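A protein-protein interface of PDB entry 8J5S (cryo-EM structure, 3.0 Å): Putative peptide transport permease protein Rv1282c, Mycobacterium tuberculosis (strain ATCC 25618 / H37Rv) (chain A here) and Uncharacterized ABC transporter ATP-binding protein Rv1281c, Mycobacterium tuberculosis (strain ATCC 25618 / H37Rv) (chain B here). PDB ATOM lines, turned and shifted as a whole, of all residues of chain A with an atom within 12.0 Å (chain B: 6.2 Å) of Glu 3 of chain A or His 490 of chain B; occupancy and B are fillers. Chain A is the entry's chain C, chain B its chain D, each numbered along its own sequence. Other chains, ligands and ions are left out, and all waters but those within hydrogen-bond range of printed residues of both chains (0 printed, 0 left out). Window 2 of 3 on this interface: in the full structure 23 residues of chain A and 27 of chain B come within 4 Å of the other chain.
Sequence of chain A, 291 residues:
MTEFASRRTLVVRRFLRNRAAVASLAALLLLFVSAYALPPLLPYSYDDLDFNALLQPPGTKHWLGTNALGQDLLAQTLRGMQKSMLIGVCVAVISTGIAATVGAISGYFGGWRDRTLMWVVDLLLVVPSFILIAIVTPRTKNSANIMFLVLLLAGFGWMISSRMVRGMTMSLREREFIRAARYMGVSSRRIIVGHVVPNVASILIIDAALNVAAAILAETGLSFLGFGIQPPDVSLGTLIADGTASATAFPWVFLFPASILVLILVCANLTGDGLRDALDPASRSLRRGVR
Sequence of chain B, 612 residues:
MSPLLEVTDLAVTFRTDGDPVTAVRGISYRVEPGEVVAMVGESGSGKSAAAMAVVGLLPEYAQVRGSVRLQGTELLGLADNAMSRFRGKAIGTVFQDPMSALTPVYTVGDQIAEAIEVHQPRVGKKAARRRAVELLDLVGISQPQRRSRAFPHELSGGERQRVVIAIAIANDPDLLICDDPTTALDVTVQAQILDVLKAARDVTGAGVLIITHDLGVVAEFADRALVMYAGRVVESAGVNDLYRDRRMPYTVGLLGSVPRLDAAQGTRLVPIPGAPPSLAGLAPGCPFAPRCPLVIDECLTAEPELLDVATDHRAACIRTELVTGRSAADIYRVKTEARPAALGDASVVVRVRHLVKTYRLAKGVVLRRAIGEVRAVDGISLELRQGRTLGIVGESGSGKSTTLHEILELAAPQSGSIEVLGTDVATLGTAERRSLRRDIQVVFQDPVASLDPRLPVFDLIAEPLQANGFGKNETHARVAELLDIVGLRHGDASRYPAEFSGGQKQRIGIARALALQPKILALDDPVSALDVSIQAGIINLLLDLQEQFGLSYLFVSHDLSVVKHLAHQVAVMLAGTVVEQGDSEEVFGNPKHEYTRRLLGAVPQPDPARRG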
ATOM      1  N   THR A   2      26.099   5.160 -15.576  1.00  0.00           N
ATOM      2  CA  THR A   2      25.510   6.245 -14.804  1.00  0.00           C
ATOM      3  C   THR A   2      26.060   7.581 -15.287  1.00  0.00           C
ATOM      4  O   THR A   2      25.372   8.602 -15.262  1.00  0.00           O
ATOM      5  CB  THR A   2      25.788   6.069 -13.303  1.00  0.00           C
ATOM      6  OG1 THR A   2      25.253   4.815 -12.866  1.00  0.00           O
ATOM      7  CG2 THR A   2      25.151   7.184 -12.497  1.00  0.00           C
ATOM      8  N   GLU A   3      27.305   7.556 -15.752  1.00  0.00           N
ATOM      9  CA  GLU A   3      28.012   8.741 -16.232  1.00  0.00           C
ATOM     10  C   GLU A   3      27.985   8.831 -17.750  1.00  0.00           C
ATOM     11  O   GLU A   3      28.970   9.224 -18.379  1.00  0.00           O
ATOM     12  CB  GLU A   3      29.447   8.747 -15.712  1.00  0.00           C
ATOM     13  CG  GLU A   3      30.219   7.459 -15.958  1.00  0.00           C
ATOM     14  CD  GLU A   3      29.971   6.406 -14.892  1.00  0.00           C
ATOM     15  OE1 GLU A   3      29.199   6.683 -13.951  1.00  0.00           O
ATOM     16  OE2 GLU A   3      30.536   5.299 -15.001  1.00  0.00           O
ATOM     17  N   PHE A   4      26.862   8.459 -18.357  1.00  0.00           N
ATOM     18  CA  PHE A   4      26.776   8.375 -19.808  1.00  0.00           C
ATOM     19  C   PHE A   4      26.881   9.754 -20.441  1.00  0.00           C
ATOM     20  O   PHE A   4      26.194  10.692 -20.030  1.00  0.00           O
ATOM     21  CB  PHE A   4      25.468   7.709 -20.209  1.00  0.00           C
ATOM     22  CG  PHE A   4      25.380   6.271 -19.808  1.00  0.00           C
ATOM     23  CD1 PHE A   4      24.676   5.888 -18.690  1.00  0.00           C
ATOM     24  CD2 PHE A   4      26.015   5.306 -20.545  1.00  0.00           C
ATOM     25  CE1 PHE A   4      24.605   4.570 -18.329  1.00  0.00           C
ATOM     26  CE2 PHE A   4      25.941   3.986 -20.189  1.00  0.00           C
ATOM     27  CZ  PHE A   4      25.238   3.618 -19.080  1.00  0.00           C
ATOM     28  N   ALA A   5      27.740   9.872 -21.446  1.00  0.00           N
ATOM     29  CA  ALA A   5      27.935  11.134 -22.138  1.00  0.00           C
ATOM     30  C   ALA A   5      26.783  11.398 -23.097  1.00  0.00           C
ATOM     31  O   ALA A   5      26.085  10.484 -23.540  1.00  0.00           O
ATOM     32  CB  ALA A   5      29.260  11.136 -22.899  1.00  0.00           C
ATOM     33  N   SER A   6      26.597  12.673 -23.423  1.00  0.00           N
ATOM     34  CA  SER A   6      25.515  13.094 -24.299  1.00  0.00           C
ATOM     35  C   SER A   6      25.901  12.836 -25.751  1.00  0.00           C
ATOM     36  O   SER A   6      26.895  12.171 -26.047  1.00  0.00           O
ATOM     37  CB  SER A   6      25.183  14.559 -24.056  1.00  0.00           C
ATOM     38  OG  SER A   6      26.024  15.387 -24.831  1.00  0.00           O
ATOM     39  N   ARG A   7      25.108  13.353 -26.682  1.00  0.00           N
ATOM     40  CA  ARG A   7      25.373  13.190 -28.104  1.00  0.00           C
ATOM     41  C   ARG A   7      25.948  14.441 -28.747  1.00  0.00           C
ATOM     42  O   ARG A   7      26.847  14.339 -29.585  1.00  0.00           O
ATOM     43  CB  ARG A   7      24.096  12.792 -28.842  1.00  0.00           C
ATOM     44  CG  ARG A   7      24.352  12.068 -30.135  1.00  0.00           C
ATOM     45  CD  ARG A   7      23.084  11.937 -30.943  1.00  0.00           C
ATOM     46  NE  ARG A   7      22.287  13.154 -30.893  1.00  0.00           N
ATOM     47  CZ  ARG A   7      22.108  13.969 -31.927  1.00  0.00           C
ATOM     48  NH1 ARG A   7      22.672  13.693 -33.092  1.00  0.00           N
ATOM     49  NH2 ARG A   7      21.367  15.057 -31.796  1.00  0.00           N
ATOM     50  N   THR A   9      27.761  16.650 -27.225  1.00  0.00           N
ATOM     51  CA  THR A   9      29.134  16.676 -26.743  1.00  0.00           C
ATOM     52  C   THR A   9      29.921  15.444 -27.154  1.00  0.00           C
ATOM     53  O   THR A   9      31.087  15.324 -26.778  1.00  0.00           O
ATOM     54  CB  THR A   9      29.171  16.825 -25.221  1.00  0.00           C
ATOM     55  OG1 THR A   9      28.963  15.553 -24.605  1.00  0.00           O
ATOM     56  CG2 THR A   9      28.099  17.789 -24.758  1.00  0.00           C
ATOM     57  N   LEU A  10      29.318  14.528 -27.902  1.00  0.00           N
ATOM     58  CA  LEU A  10      30.038  13.396 -28.459  1.00  0.00           C
ATOM     59  C   LEU A  10      30.500  13.633 -29.887  1.00  0.00           C
ATOM     60  O   LEU A  10      31.395  12.925 -30.357  1.00  0.00           O
ATOM     61  CB  LEU A  10      29.163  12.138 -28.414  1.00  0.00           C
ATOM     62  CG  LEU A  10      29.855  10.792 -28.237  1.00  0.00           C
ATOM     63  CD1 LEU A  10      30.763  10.815 -27.030  1.00  0.00           C
ATOM     64  CD2 LEU A  10      28.826   9.700 -28.101  1.00  0.00           C
ATOM     65  N   ARG A  13      33.661  16.551 -29.841  1.00  0.00           N
ATOM     66  CA  ARG A  13      34.960  15.981 -29.508  1.00  0.00           C
ATOM     67  C   ARG A  13      35.567  15.268 -30.706  1.00  0.00           C
ATOM     68  O   ARG A  13      36.790  15.327 -30.925  1.00  0.00           O
ATOM     69  CB  ARG A  13      34.809  15.044 -28.311  1.00  0.00           C
ATOM     70  CG  ARG A  13      34.187  15.726 -27.098  1.00  0.00           C
ATOM     71  CD  ARG A  13      34.063  14.793 -25.908  1.00  0.00           C
ATOM     72  NE  ARG A  13      35.361  14.297 -25.474  1.00  0.00           N
ATOM     73  CZ  ARG A  13      35.769  13.043 -25.630  1.00  0.00           C
ATOM     74  NH1 ARG A  13      34.977  12.153 -26.213  1.00  0.00           N
ATOM     75  NH2 ARG A  13      36.970  12.679 -25.205  1.00  0.00           N
ATOM     76  N   HIS B 476      19.820   7.557 -16.487  1.00  0.00           N
ATOM     77  CA  HIS B 476      21.187   7.008 -16.608  1.00  0.00           C
ATOM     78  C   HIS B 476      21.280   5.733 -15.775  1.00  0.00           C
ATOM     79  O   HIS B 476      21.981   4.718 -16.169  1.00  0.00           O
ATOM     80  CB  HIS B 476      22.157   8.080 -16.129  1.00  0.00           C
ATOM     81  CG  HIS B 476      22.083   9.345 -16.913  1.00  0.00           C
ATOM     82  ND1 HIS B 476      21.410  10.459 -16.469  1.00  0.00           N
ATOM     83  CD2 HIS B 476      22.594   9.672 -18.102  1.00  0.00           C
ATOM     84  CE1 HIS B 476      21.515  11.418 -17.374  1.00  0.00           C
ATOM     85  NE2 HIS B 476      22.232  10.961 -18.373  1.00  0.00           N
ATOM     86  N   LEU B 483      22.070  -2.434 -19.599  1.00  0.00           N
ATOM     87  CA  LEU B 483      23.070  -2.947 -20.527  1.00  0.00           C
ATOM     88  C   LEU B 483      24.094  -3.859 -19.866  1.00  0.00           C
ATOM     89  O   LEU B 483      24.956  -4.393 -20.558  1.00  0.00           O
ATOM     90  CB  LEU B 483      23.767  -1.805 -21.275  1.00  0.00           C
ATOM     91  CG  LEU B 483      24.917  -0.952 -20.762  1.00  0.00           C
ATOM     92  CD1 LEU B 483      25.386  -0.076 -21.892  1.00  0.00           C
ATOM     93  CD2 LEU B 483      24.529  -0.099 -19.613  1.00  0.00           C
ATOM     94  N   ASP B 484      24.009  -4.079 -18.559  1.00  0.00           N
ATOM     95  CA  ASP B 484      24.738  -5.183 -17.950  1.00  0.00           C
ATOM     96  C   ASP B 484      23.926  -6.461 -17.934  1.00  0.00           C
ATOM     97  O   ASP B 484      24.503  -7.552 -17.957  1.00  0.00           O
ATOM     98  CB  ASP B 484      25.149  -4.854 -16.516  1.00  0.00           C
ATOM     99  CG  ASP B 484      25.774  -3.493 -16.389  1.00  0.00           C
ATOM    100  OD1 ASP B 484      25.602  -2.862 -15.325  1.00  0.00           O
ATOM    101  OD2 ASP B 484      26.440  -3.053 -17.346  1.00  0.00           O
ATOM    102  N   LEU B 488      26.165  -5.844 -22.419  1.00  0.00           N
ATOM    103  CA  LEU B 488      26.940  -4.734 -22.949  1.00  0.00           C
ATOM    104  C   LEU B 488      27.746  -4.085 -21.819  1.00  0.00           C
ATOM    105  O   LEU B 488      27.756  -4.551 -20.680  1.00  0.00           O
ATOM    106  CB  LEU B 488      26.012  -3.733 -23.631  1.00  0.00           C
ATOM    107  CG  LEU B 488      25.153  -4.244 -24.790  1.00  0.00           C
ATOM    108  CD1 LEU B 488      24.750  -3.090 -25.684  1.00  0.00           C
ATOM    109  CD2 LEU B 488      25.889  -5.291 -25.589  1.00  0.00           C
ATOM    110  N   ARG B 489      28.456  -3.007 -22.137  1.00  0.00           N
ATOM    111  CA  ARG B 489      29.311  -2.336 -21.168  1.00  0.00           C
ATOM    112  C   ARG B 489      29.091  -0.833 -21.257  1.00  0.00           C
ATOM    113  O   ARG B 489      28.641  -0.311 -22.281  1.00  0.00           O
ATOM    114  CB  ARG B 489      30.793  -2.677 -21.411  1.00  0.00           C
ATOM    115  CG  ARG B 489      30.999  -4.017 -22.105  1.00  0.00           C
ATOM    116  CD  ARG B 489      32.382  -4.571 -21.896  1.00  0.00           C
ATOM    117  NE  ARG B 489      32.582  -5.015 -20.523  1.00  0.00           N
ATOM    118  CZ  ARG B 489      32.164  -6.178 -20.037  1.00  0.00           C
ATOM    119  NH1 ARG B 489      31.509  -7.035 -20.808  1.00  0.00           N
ATOM    120  NH2 ARG B 489      32.401  -6.485 -18.772  1.00  0.00           N
ATOM    121  N   HIS B 490      29.416  -0.137 -20.166  1.00  0.00           N
ATOM    122  CA  HIS B 490      29.133   1.292 -20.082  1.00  0.00           C
ATOM    123  C   HIS B 490      29.805   2.061 -21.209  1.00  0.00           C
ATOM    124  O   HIS B 490      29.272   3.077 -21.669  1.00  0.00           O
ATOM    125  CB  HIS B 490      29.566   1.831 -18.713  1.00  0.00           C
ATOM    126  CG  HIS B 490      29.481   3.321 -18.583  1.00  0.00           C
ATOM    127  ND1 HIS B 490      30.238   4.186 -19.343  1.00  0.00           N
ATOM    128  CD2 HIS B 490      28.733   4.100 -17.766  1.00  0.00           C
ATOM    129  CE1 HIS B 490      29.953   5.432 -19.009  1.00  0.00           C
ATOM    130  NE2 HIS B 490      29.044   5.406 -18.054  1.00  0.00           N
ATOM    131  N   GLY B 491      30.969   1.602 -21.659  1.00  0.00           N
ATOM    132  CA  GLY B 491      31.643   2.275 -22.752  1.00  0.00           C
ATOM    133  C   GLY B 491      30.901   2.157 -24.068  1.00  0.00           C
ATOM    134  O   GLY B 491      30.851   3.115 -24.844  1.00  0.00           O
ATOM    135  N   ASP B 492      30.295   0.993 -24.327  1.00  0.00           N
ATOM    136  CA  ASP B 492      29.583   0.788 -25.586  1.00  0.00           C
ATOM    137  C   ASP B 492      28.521   1.843 -25.807  1.00  0.00           C
ATOM    138  O   ASP B 492      28.155   2.124 -26.951  1.00  0.00           O
ATOM    139  CB  ASP B 492      28.906  -0.578 -25.631  1.00  0.00           C
ATOM    140  CG  ASP B 492      29.807  -1.695 -25.199  1.00  0.00           C
ATOM    141  OD1 ASP B 492      29.583  -2.217 -24.107  1.00  0.00           O
ATOM    142  OD2 ASP B 492      30.722  -2.072 -25.954  1.00  0.00           O
ATOM    143  N   ALA B 493      28.006   2.427 -24.728  1.00  0.00           N
ATOM    144  CA  ALA B 493      26.971   3.439 -24.852  1.00  0.00           C
ATOM    145  C   ALA B 493      27.399   4.572 -25.767  1.00  0.00           C
ATOM    146  O   ALA B 493      26.601   5.068 -26.568  1.00  0.00           O
ATOM    147  CB  ALA B 493      26.611   3.976 -23.480  1.00  0.00           C
ATOM    148  N   SER B 494      28.652   4.989 -25.675  1.00  0.00           N
ATOM    149  CA  SER B 494      29.148   6.036 -26.551  1.00  0.00           C
ATOM    150  C   SER B 494      29.417   5.549 -27.967  1.00  0.00           C
ATOM    151  O   SER B 494      29.722   6.367 -28.837  1.00  0.00           O
ATOM    152  CB  SER B 494      30.414   6.642 -25.959  1.00  0.00           C
ATOM    153  OG  SER B 494      30.179   7.077 -24.633  1.00  0.00           O
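The backbone NH (N) of Leu 488 of chain B sits at hydrogen-bond distance from the backbone carbonyl oxygen (O) of Leu 483 of chain B, at 2.7 Å.
Of chain B, only His 490 comes within 4 Å of Glu 3 of chain A.
His 490 of chain B touches just these residues of chain A: Thr 2, Glu 3 and Phe 4.
Of chain A, only Thr 2 and Phe 4 come within 4 Å of His 476 of chain B.
No residue of chain A comes within 4 Å of Arg 489 of chain B.
Asp 492 of chain B touches none of the printed residues of chain A.
Ala 493 of chain B touches just one residue of chain A: Phe 4 (3.3 Å).
Of the printed residues of chain B, Leu 10 of chain A touches Ser 494 (3.5 Å).
Printed residues of chain B within 4 Å of Phe 4 of chain A: His 476 (3.4 Å), Leu 483 (3.8 Å), His 490 (3.7 Å) and Ala 493 (3.3 Å).
Of the printed residues of chain B, Thr 2 of chain A touches His 476 and His 490.
A ring nitrogen (NE2) of His 490 of chain B lies close to the side-chain carboxylate (OE2) of Glu 3 of chain A, at 3.4 Å.
Among the printed residues, pairs that only touch across the chains: Phe 4 of chain A with Ala 493 of chain B (3.3 Å), Thr 2 of chain A with His 476 of chain B (3.4 Å), Phe 4 of chain A with His 476 of chain B (3.4 Å), Leu 10 of chain A with Ser 494 of chain B (3.5 Å), Thr 2 of chain A with His 490 of chain B (3.6 Å), Phe 4 of chain A with His 490 of chain B (3.7 Å) and Phe 4 of chain A with Leu 483 of chain B (3.8 Å).
Of the 9 printed residues of chain A, 4 touch a printed residue of chain B.
Printed residues of chain A that touch a printed residue of chain B: Thr 2, Glu 3, Phe 4 and Leu 10.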
